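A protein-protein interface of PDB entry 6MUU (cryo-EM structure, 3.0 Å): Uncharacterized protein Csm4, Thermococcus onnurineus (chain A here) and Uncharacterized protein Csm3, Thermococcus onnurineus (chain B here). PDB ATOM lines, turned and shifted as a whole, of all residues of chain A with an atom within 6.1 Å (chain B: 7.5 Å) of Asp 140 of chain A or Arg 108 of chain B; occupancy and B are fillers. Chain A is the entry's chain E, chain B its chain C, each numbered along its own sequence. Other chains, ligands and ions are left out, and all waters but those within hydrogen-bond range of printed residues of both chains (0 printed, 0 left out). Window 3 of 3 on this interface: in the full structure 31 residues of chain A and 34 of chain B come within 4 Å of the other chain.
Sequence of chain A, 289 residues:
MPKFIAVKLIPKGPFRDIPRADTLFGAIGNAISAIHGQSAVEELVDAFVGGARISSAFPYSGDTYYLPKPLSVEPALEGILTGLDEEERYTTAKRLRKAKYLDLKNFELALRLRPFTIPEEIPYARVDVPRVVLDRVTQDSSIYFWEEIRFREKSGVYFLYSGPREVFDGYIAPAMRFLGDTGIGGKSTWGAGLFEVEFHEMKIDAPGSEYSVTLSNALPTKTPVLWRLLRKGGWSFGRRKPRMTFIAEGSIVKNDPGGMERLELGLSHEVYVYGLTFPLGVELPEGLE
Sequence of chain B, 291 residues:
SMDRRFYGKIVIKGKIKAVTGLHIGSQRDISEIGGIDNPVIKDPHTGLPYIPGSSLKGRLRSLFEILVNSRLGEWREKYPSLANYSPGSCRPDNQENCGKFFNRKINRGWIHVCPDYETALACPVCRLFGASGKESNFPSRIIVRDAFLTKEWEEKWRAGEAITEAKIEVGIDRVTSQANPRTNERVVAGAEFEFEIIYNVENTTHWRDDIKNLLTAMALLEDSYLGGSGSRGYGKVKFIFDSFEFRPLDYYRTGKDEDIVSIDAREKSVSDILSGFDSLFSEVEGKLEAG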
ATOM      1  N   VAL A 132     -14.328  -3.391 -27.488  1.00  0.00           N
ATOM      2  CA  VAL A 132     -13.863  -2.050 -27.798  1.00  0.00           C
ATOM      3  C   VAL A 132     -15.008  -1.283 -28.441  1.00  0.00           C
ATOM      4  O   VAL A 132     -15.978  -1.861 -28.924  1.00  0.00           O
ATOM      5  CB  VAL A 132     -12.607  -2.073 -28.703  1.00  0.00           C
ATOM      6  CG1 VAL A 132     -12.955  -2.156 -30.151  1.00  0.00           C
ATOM      7  CG2 VAL A 132     -11.719  -0.919 -28.425  1.00  0.00           C
ATOM      8  N   VAL A 133     -14.917   0.039 -28.376  1.00  0.00           N
ATOM      9  CA  VAL A 133     -15.813   0.952 -29.070  1.00  0.00           C
ATOM     10  C   VAL A 133     -14.952   1.841 -29.942  1.00  0.00           C
ATOM     11  O   VAL A 133     -14.036   2.502 -29.442  1.00  0.00           O
ATOM     12  CB  VAL A 133     -16.641   1.792 -28.094  1.00  0.00           C
ATOM     13  CG1 VAL A 133     -17.336   2.887 -28.823  1.00  0.00           C
ATOM     14  CG2 VAL A 133     -17.645   0.941 -27.436  1.00  0.00           C
ATOM     15  N   LEU A 134     -15.227   1.855 -31.237  1.00  0.00           N
ATOM     16  CA  LEU A 134     -14.418   2.618 -32.167  1.00  0.00           C
ATOM     17  C   LEU A 134     -15.178   3.825 -32.687  1.00  0.00           C
ATOM     18  O   LEU A 134     -16.357   3.725 -33.032  1.00  0.00           O
ATOM     19  CB  LEU A 134     -13.965   1.751 -33.333  1.00  0.00           C
ATOM     20  CG  LEU A 134     -13.060   0.600 -32.913  1.00  0.00           C
ATOM     21  CD1 LEU A 134     -12.648  -0.180 -34.101  1.00  0.00           C
ATOM     22  CD2 LEU A 134     -11.848   1.100 -32.200  1.00  0.00           C
ATOM     23  N   ASP A 135     -14.499   4.966 -32.712  1.00  0.00           N
ATOM     24  CA  ASP A 135     -14.989   6.104 -33.469  1.00  0.00           C
ATOM     25  C   ASP A 135     -15.021   5.744 -34.942  1.00  0.00           C
ATOM     26  O   ASP A 135     -14.122   5.069 -35.448  1.00  0.00           O
ATOM     27  CB  ASP A 135     -14.098   7.319 -33.244  1.00  0.00           C
ATOM     28  CG  ASP A 135     -14.604   8.553 -33.951  1.00  0.00           C
ATOM     29  OD1 ASP A 135     -15.612   9.132 -33.505  1.00  0.00           O
ATOM     30  OD2 ASP A 135     -13.986   8.954 -34.955  1.00  0.00           O
ATOM     31  N   THR A 138     -12.280   8.619 -36.820  1.00  0.00           N
ATOM     32  CA  THR A 138     -10.913   8.617 -36.312  1.00  0.00           C
ATOM     33  C   THR A 138     -10.818   7.516 -35.270  1.00  0.00           C
ATOM     34  O   THR A 138     -11.037   7.791 -34.088  1.00  0.00           O
ATOM     35  CB  THR A 138     -10.589   9.953 -35.678  1.00  0.00           C
ATOM     36  OG1 THR A 138     -11.438  10.136 -34.542  1.00  0.00           O
ATOM     37  CG2 THR A 138     -10.824  11.083 -36.641  1.00  0.00           C
ATOM     38  N   GLN A 139     -10.396   6.313 -35.673  1.00  0.00           N
ATOM     39  CA  GLN A 139     -10.773   5.077 -34.979  1.00  0.00           C
ATOM     40  C   GLN A 139     -10.120   4.988 -33.605  1.00  0.00           C
ATOM     41  O   GLN A 139      -9.160   4.251 -33.372  1.00  0.00           O
ATOM     42  CB  GLN A 139     -10.416   3.868 -35.826  1.00  0.00           C
ATOM     43  CG  GLN A 139     -11.171   3.819 -37.121  1.00  0.00           C
ATOM     44  CD  GLN A 139     -10.870   2.584 -37.927  1.00  0.00           C
ATOM     45  OE1 GLN A 139     -10.084   1.738 -37.518  1.00  0.00           O
ATOM     46  NE2 GLN A 139     -11.490   2.477 -39.090  1.00  0.00           N
ATOM     47  N   ASP A 140     -10.685   5.754 -32.673  1.00  0.00           N
ATOM     48  CA  ASP A 140     -10.215   5.798 -31.300  1.00  0.00           C
ATOM     49  C   ASP A 140     -10.795   4.637 -30.521  1.00  0.00           C
ATOM     50  O   ASP A 140     -12.015   4.490 -30.428  1.00  0.00           O
ATOM     51  CB  ASP A 140     -10.624   7.102 -30.625  1.00  0.00           C
ATOM     52  CG  ASP A 140      -9.940   8.298 -31.213  1.00  0.00           C
ATOM     53  OD1 ASP A 140      -8.829   8.132 -31.747  1.00  0.00           O
ATOM     54  OD2 ASP A 140     -10.511   9.404 -31.143  1.00  0.00           O
ATOM     55  N   SER A 141      -9.925   3.837 -29.931  1.00  0.00           N
ATOM     56  CA  SER A 141     -10.337   2.675 -29.170  1.00  0.00           C
ATOM     57  C   SER A 141     -10.637   3.095 -27.741  1.00  0.00           C
ATOM     58  O   SER A 141      -9.880   3.867 -27.145  1.00  0.00           O
ATOM     59  CB  SER A 141      -9.244   1.610 -29.194  1.00  0.00           C
ATOM     60  OG  SER A 141      -8.085   2.053 -28.519  1.00  0.00           O
ATOM     61  N   SER A 142     -11.745   2.598 -27.200  1.00  0.00           N
ATOM     62  CA  SER A 142     -12.135   2.888 -25.823  1.00  0.00           C
ATOM     63  C   SER A 142     -12.771   1.629 -25.251  1.00  0.00           C
ATOM     64  O   SER A 142     -13.947   1.364 -25.498  1.00  0.00           O
ATOM     65  CB  SER A 142     -13.089   4.070 -25.761  1.00  0.00           C
ATOM     66  OG  SER A 142     -14.320   3.755 -26.373  1.00  0.00           O
ATOM     67  N   ARG B  91     -17.871  15.254 -33.193  1.00  0.00           N
ATOM     68  CA  ARG B  91     -16.613  15.450 -32.480  1.00  0.00           C
ATOM     69  C   ARG B  91     -16.077  16.893 -32.447  1.00  0.00           C
ATOM     70  O   ARG B  91     -15.565  17.281 -31.388  1.00  0.00           O
ATOM     71  CB  ARG B  91     -15.548  14.495 -33.039  1.00  0.00           C
ATOM     72  CG  ARG B  91     -14.260  14.488 -32.231  1.00  0.00           C
ATOM     73  CD  ARG B  91     -13.269  13.441 -32.664  1.00  0.00           C
ATOM     74  NE  ARG B  91     -12.049  13.558 -31.873  1.00  0.00           N
ATOM     75  CZ  ARG B  91     -11.014  12.732 -31.961  1.00  0.00           C
ATOM     76  NH1 ARG B  91      -9.944  12.919 -31.205  1.00  0.00           N
ATOM     77  NH2 ARG B  91     -11.054  11.711 -32.797  1.00  0.00           N
ATOM     78  N   LYS B 105     -21.954   9.566 -28.449  1.00  0.00           N
ATOM     79  CA  LYS B 105     -20.615   9.335 -27.923  1.00  0.00           C
ATOM     80  C   LYS B 105     -20.696   8.311 -26.804  1.00  0.00           C
ATOM     81  O   LYS B 105     -21.410   8.524 -25.820  1.00  0.00           O
ATOM     82  CB  LYS B 105     -19.993  10.622 -27.394  1.00  0.00           C
ATOM     83  CG  LYS B 105     -18.600  10.417 -26.852  1.00  0.00           C
ATOM     84  CD  LYS B 105     -18.026  11.690 -26.275  1.00  0.00           C
ATOM     85  CE  LYS B 105     -16.606  11.477 -25.789  1.00  0.00           C
ATOM     86  NZ  LYS B 105     -16.004  12.711 -25.220  1.00  0.00           N
ATOM     87  N   ILE B 106     -19.966   7.207 -26.944  1.00  0.00           N
ATOM     88  CA  ILE B 106     -20.026   6.177 -25.919  1.00  0.00           C
ATOM     89  C   ILE B 106     -19.025   6.502 -24.824  1.00  0.00           C
ATOM     90  O   ILE B 106     -19.411   6.856 -23.704  1.00  0.00           O
ATOM     91  CB  ILE B 106     -19.753   4.784 -26.508  1.00  0.00           C
ATOM     92  CG1 ILE B 106     -20.735   4.480 -27.637  1.00  0.00           C
ATOM     93  CG2 ILE B 106     -19.854   3.731 -25.431  1.00  0.00           C
ATOM     94  CD1 ILE B 106     -22.174   4.455 -27.215  1.00  0.00           C
ATOM     95  N   ASN B 107     -17.739   6.409 -25.136  1.00  0.00           N
ATOM     96  CA  ASN B 107     -16.706   6.770 -24.178  1.00  0.00           C
ATOM     97  C   ASN B 107     -15.763   7.827 -24.722  1.00  0.00           C
ATOM     98  O   ASN B 107     -15.543   8.855 -24.077  1.00  0.00           O
ATOM     99  CB  ASN B 107     -15.929   5.511 -23.773  1.00  0.00           C
ATOM    100  CG  ASN B 107     -15.123   5.698 -22.512  1.00  0.00           C
ATOM    101  OD1 ASN B 107     -15.138   6.761 -21.896  1.00  0.00           O
ATOM    102  ND2 ASN B 107     -14.408   4.655 -22.120  1.00  0.00           N
ATOM    103  N   ARG B 108     -15.187   7.582 -25.890  1.00  0.00           N
ATOM    104  CA  ARG B 108     -14.255   8.504 -26.510  1.00  0.00           C
ATOM    105  C   ARG B 108     -14.477   8.563 -28.017  1.00  0.00           C
ATOM    106  O   ARG B 108     -13.828   9.362 -28.698  1.00  0.00           O
ATOM    107  CB  ARG B 108     -12.814   8.078 -26.149  1.00  0.00           C
ATOM    108  CG  ARG B 108     -11.699   9.095 -26.350  1.00  0.00           C
ATOM    109  CD  ARG B 108     -10.439   8.660 -25.610  1.00  0.00           C
ATOM    110  NE  ARG B 108      -9.824   7.446 -26.132  1.00  0.00           N
ATOM    111  CZ  ARG B 108      -8.894   7.430 -27.080  1.00  0.00           C
ATOM    112  NH1 ARG B 108      -8.460   8.569 -27.605  1.00  0.00           N
ATOM    113  NH2 ARG B 108      -8.386   6.279 -27.491  1.00  0.00           N
ATOM    114  N   GLY B 109     -15.414   7.775 -28.550  1.00  0.00           N
ATOM    115  CA  GLY B 109     -15.663   7.744 -29.971  1.00  0.00           C
ATOM    116  C   GLY B 109     -17.133   7.956 -30.273  1.00  0.00           C
ATOM    117  O   GLY B 109     -17.998   7.765 -29.425  1.00  0.00           O
ATOM    118  N   TRP B 110     -17.397   8.347 -31.514  1.00  0.00           N
ATOM    119  CA  TRP B 110     -18.706   8.820 -31.936  1.00  0.00           C
ATOM    120  C   TRP B 110     -19.337   7.823 -32.899  1.00  0.00           C
ATOM    121  O   TRP B 110     -18.691   7.372 -33.848  1.00  0.00           O
ATOM    122  CB  TRP B 110     -18.581  10.206 -32.570  1.00  0.00           C
ATOM    123  CG  TRP B 110     -18.121  11.223 -31.574  1.00  0.00           C
ATOM    124  CD1 TRP B 110     -16.833  11.524 -31.257  1.00  0.00           C
ATOM    125  CD2 TRP B 110     -18.938  12.089 -30.783  1.00  0.00           C
ATOM    126  NE1 TRP B 110     -16.795  12.501 -30.301  1.00  0.00           N
ATOM    127  CE2 TRP B 110     -18.077  12.866 -29.993  1.00  0.00           C
ATOM    128  CE3 TRP B 110     -20.314  12.276 -30.659  1.00  0.00           C
ATOM    129  CZ2 TRP B 110     -18.544  13.817 -29.102  1.00  0.00           C
ATOM    130  CZ3 TRP B 110     -20.774  13.215 -29.766  1.00  0.00           C
ATOM    131  CH2 TRP B 110     -19.894  13.971 -28.999  1.00  0.00           C
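NH2 of Arg 91 of chain B lies close to OG1 of Thr 138 of chain A, at 2.4 Å.
The backbone NH (N) of Trp 110 of chain B lies within hydrogen-bond range of the side-chain carboxylate (OD1) of Asp 135 of chain A (2.8 Å).
O of Ser 141 of chain A is in hydrogen-bond range of NH2 of Arg 108 of chain B (2.9 Å).
OD2 of Asp 140 of chain A is in salt-bridge range of NH2 of Arg 91 of chain B.
The backbone NH of Ser 142 of chain A lies within hydrogen-bond range of the backbone carbonyl oxygen of Val 133 of chain A, at 3.2 Å.
O of Asp 140 of chain A sits at hydrogen-bond distance from N of Asp 135 of chain A (3.4 Å).
OD2 of Asp 135 of chain A is in hydrogen-bond range of N of Thr 138 of chain A, 2.5 Å away.
Val 133 of chain A touches Ile 106 of chain B (CG1 to CB, 3.8 Å).
Gly 109 of chain B touches Asp 135 of chain A.
Asp 140 of chain A touches Arg 108 of chain B (CG to NH1, 3.9 Å).
OG of Ser 142 of chain A touches CB of Asn 107 of chain B (3.5 Å).
Ser 142 of chain A touches Arg 108 of chain B.
Val 132 of chain A touches none of the printed residues of chain B.
Leu 134 of chain A touches none of the printed residues of chain B.
Asp 140 of chain A touches just these residues of chain B: Arg 91 (2.9 Å) and Arg 108 (3.9 Å).
Of the printed residues of chain A, Ile 106 of chain B touches Val 133 (3.8 Å).
Arg 108 of chain B touches just these residues of chain A: Asp 140, Ser 141 and Ser 142.
Printed residues of chain A within 4 Å of Trp 110 of chain B: Asp 135.
The nearest residue of chain B that does not touch Asp 140 of chain A is Gly 109 of chain B (4.9 Å).
The nearest printed residue of chain B that does not touch Asp 135 of chain A is Arg 91 of chain B (4.6 Å).
Hydrophobic or aromatic side chains of chain A that line the printed part of chain B: Val 133.
Of the 7 printed residues of chain B, 6 touch a printed residue of chain A.
Hydrophobic or aromatic side chains of chain B within 4 Å of the printed part of chain A: Ile 106 and Trp 110.
Among the printed residues, 9 pairs touch across the chains.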
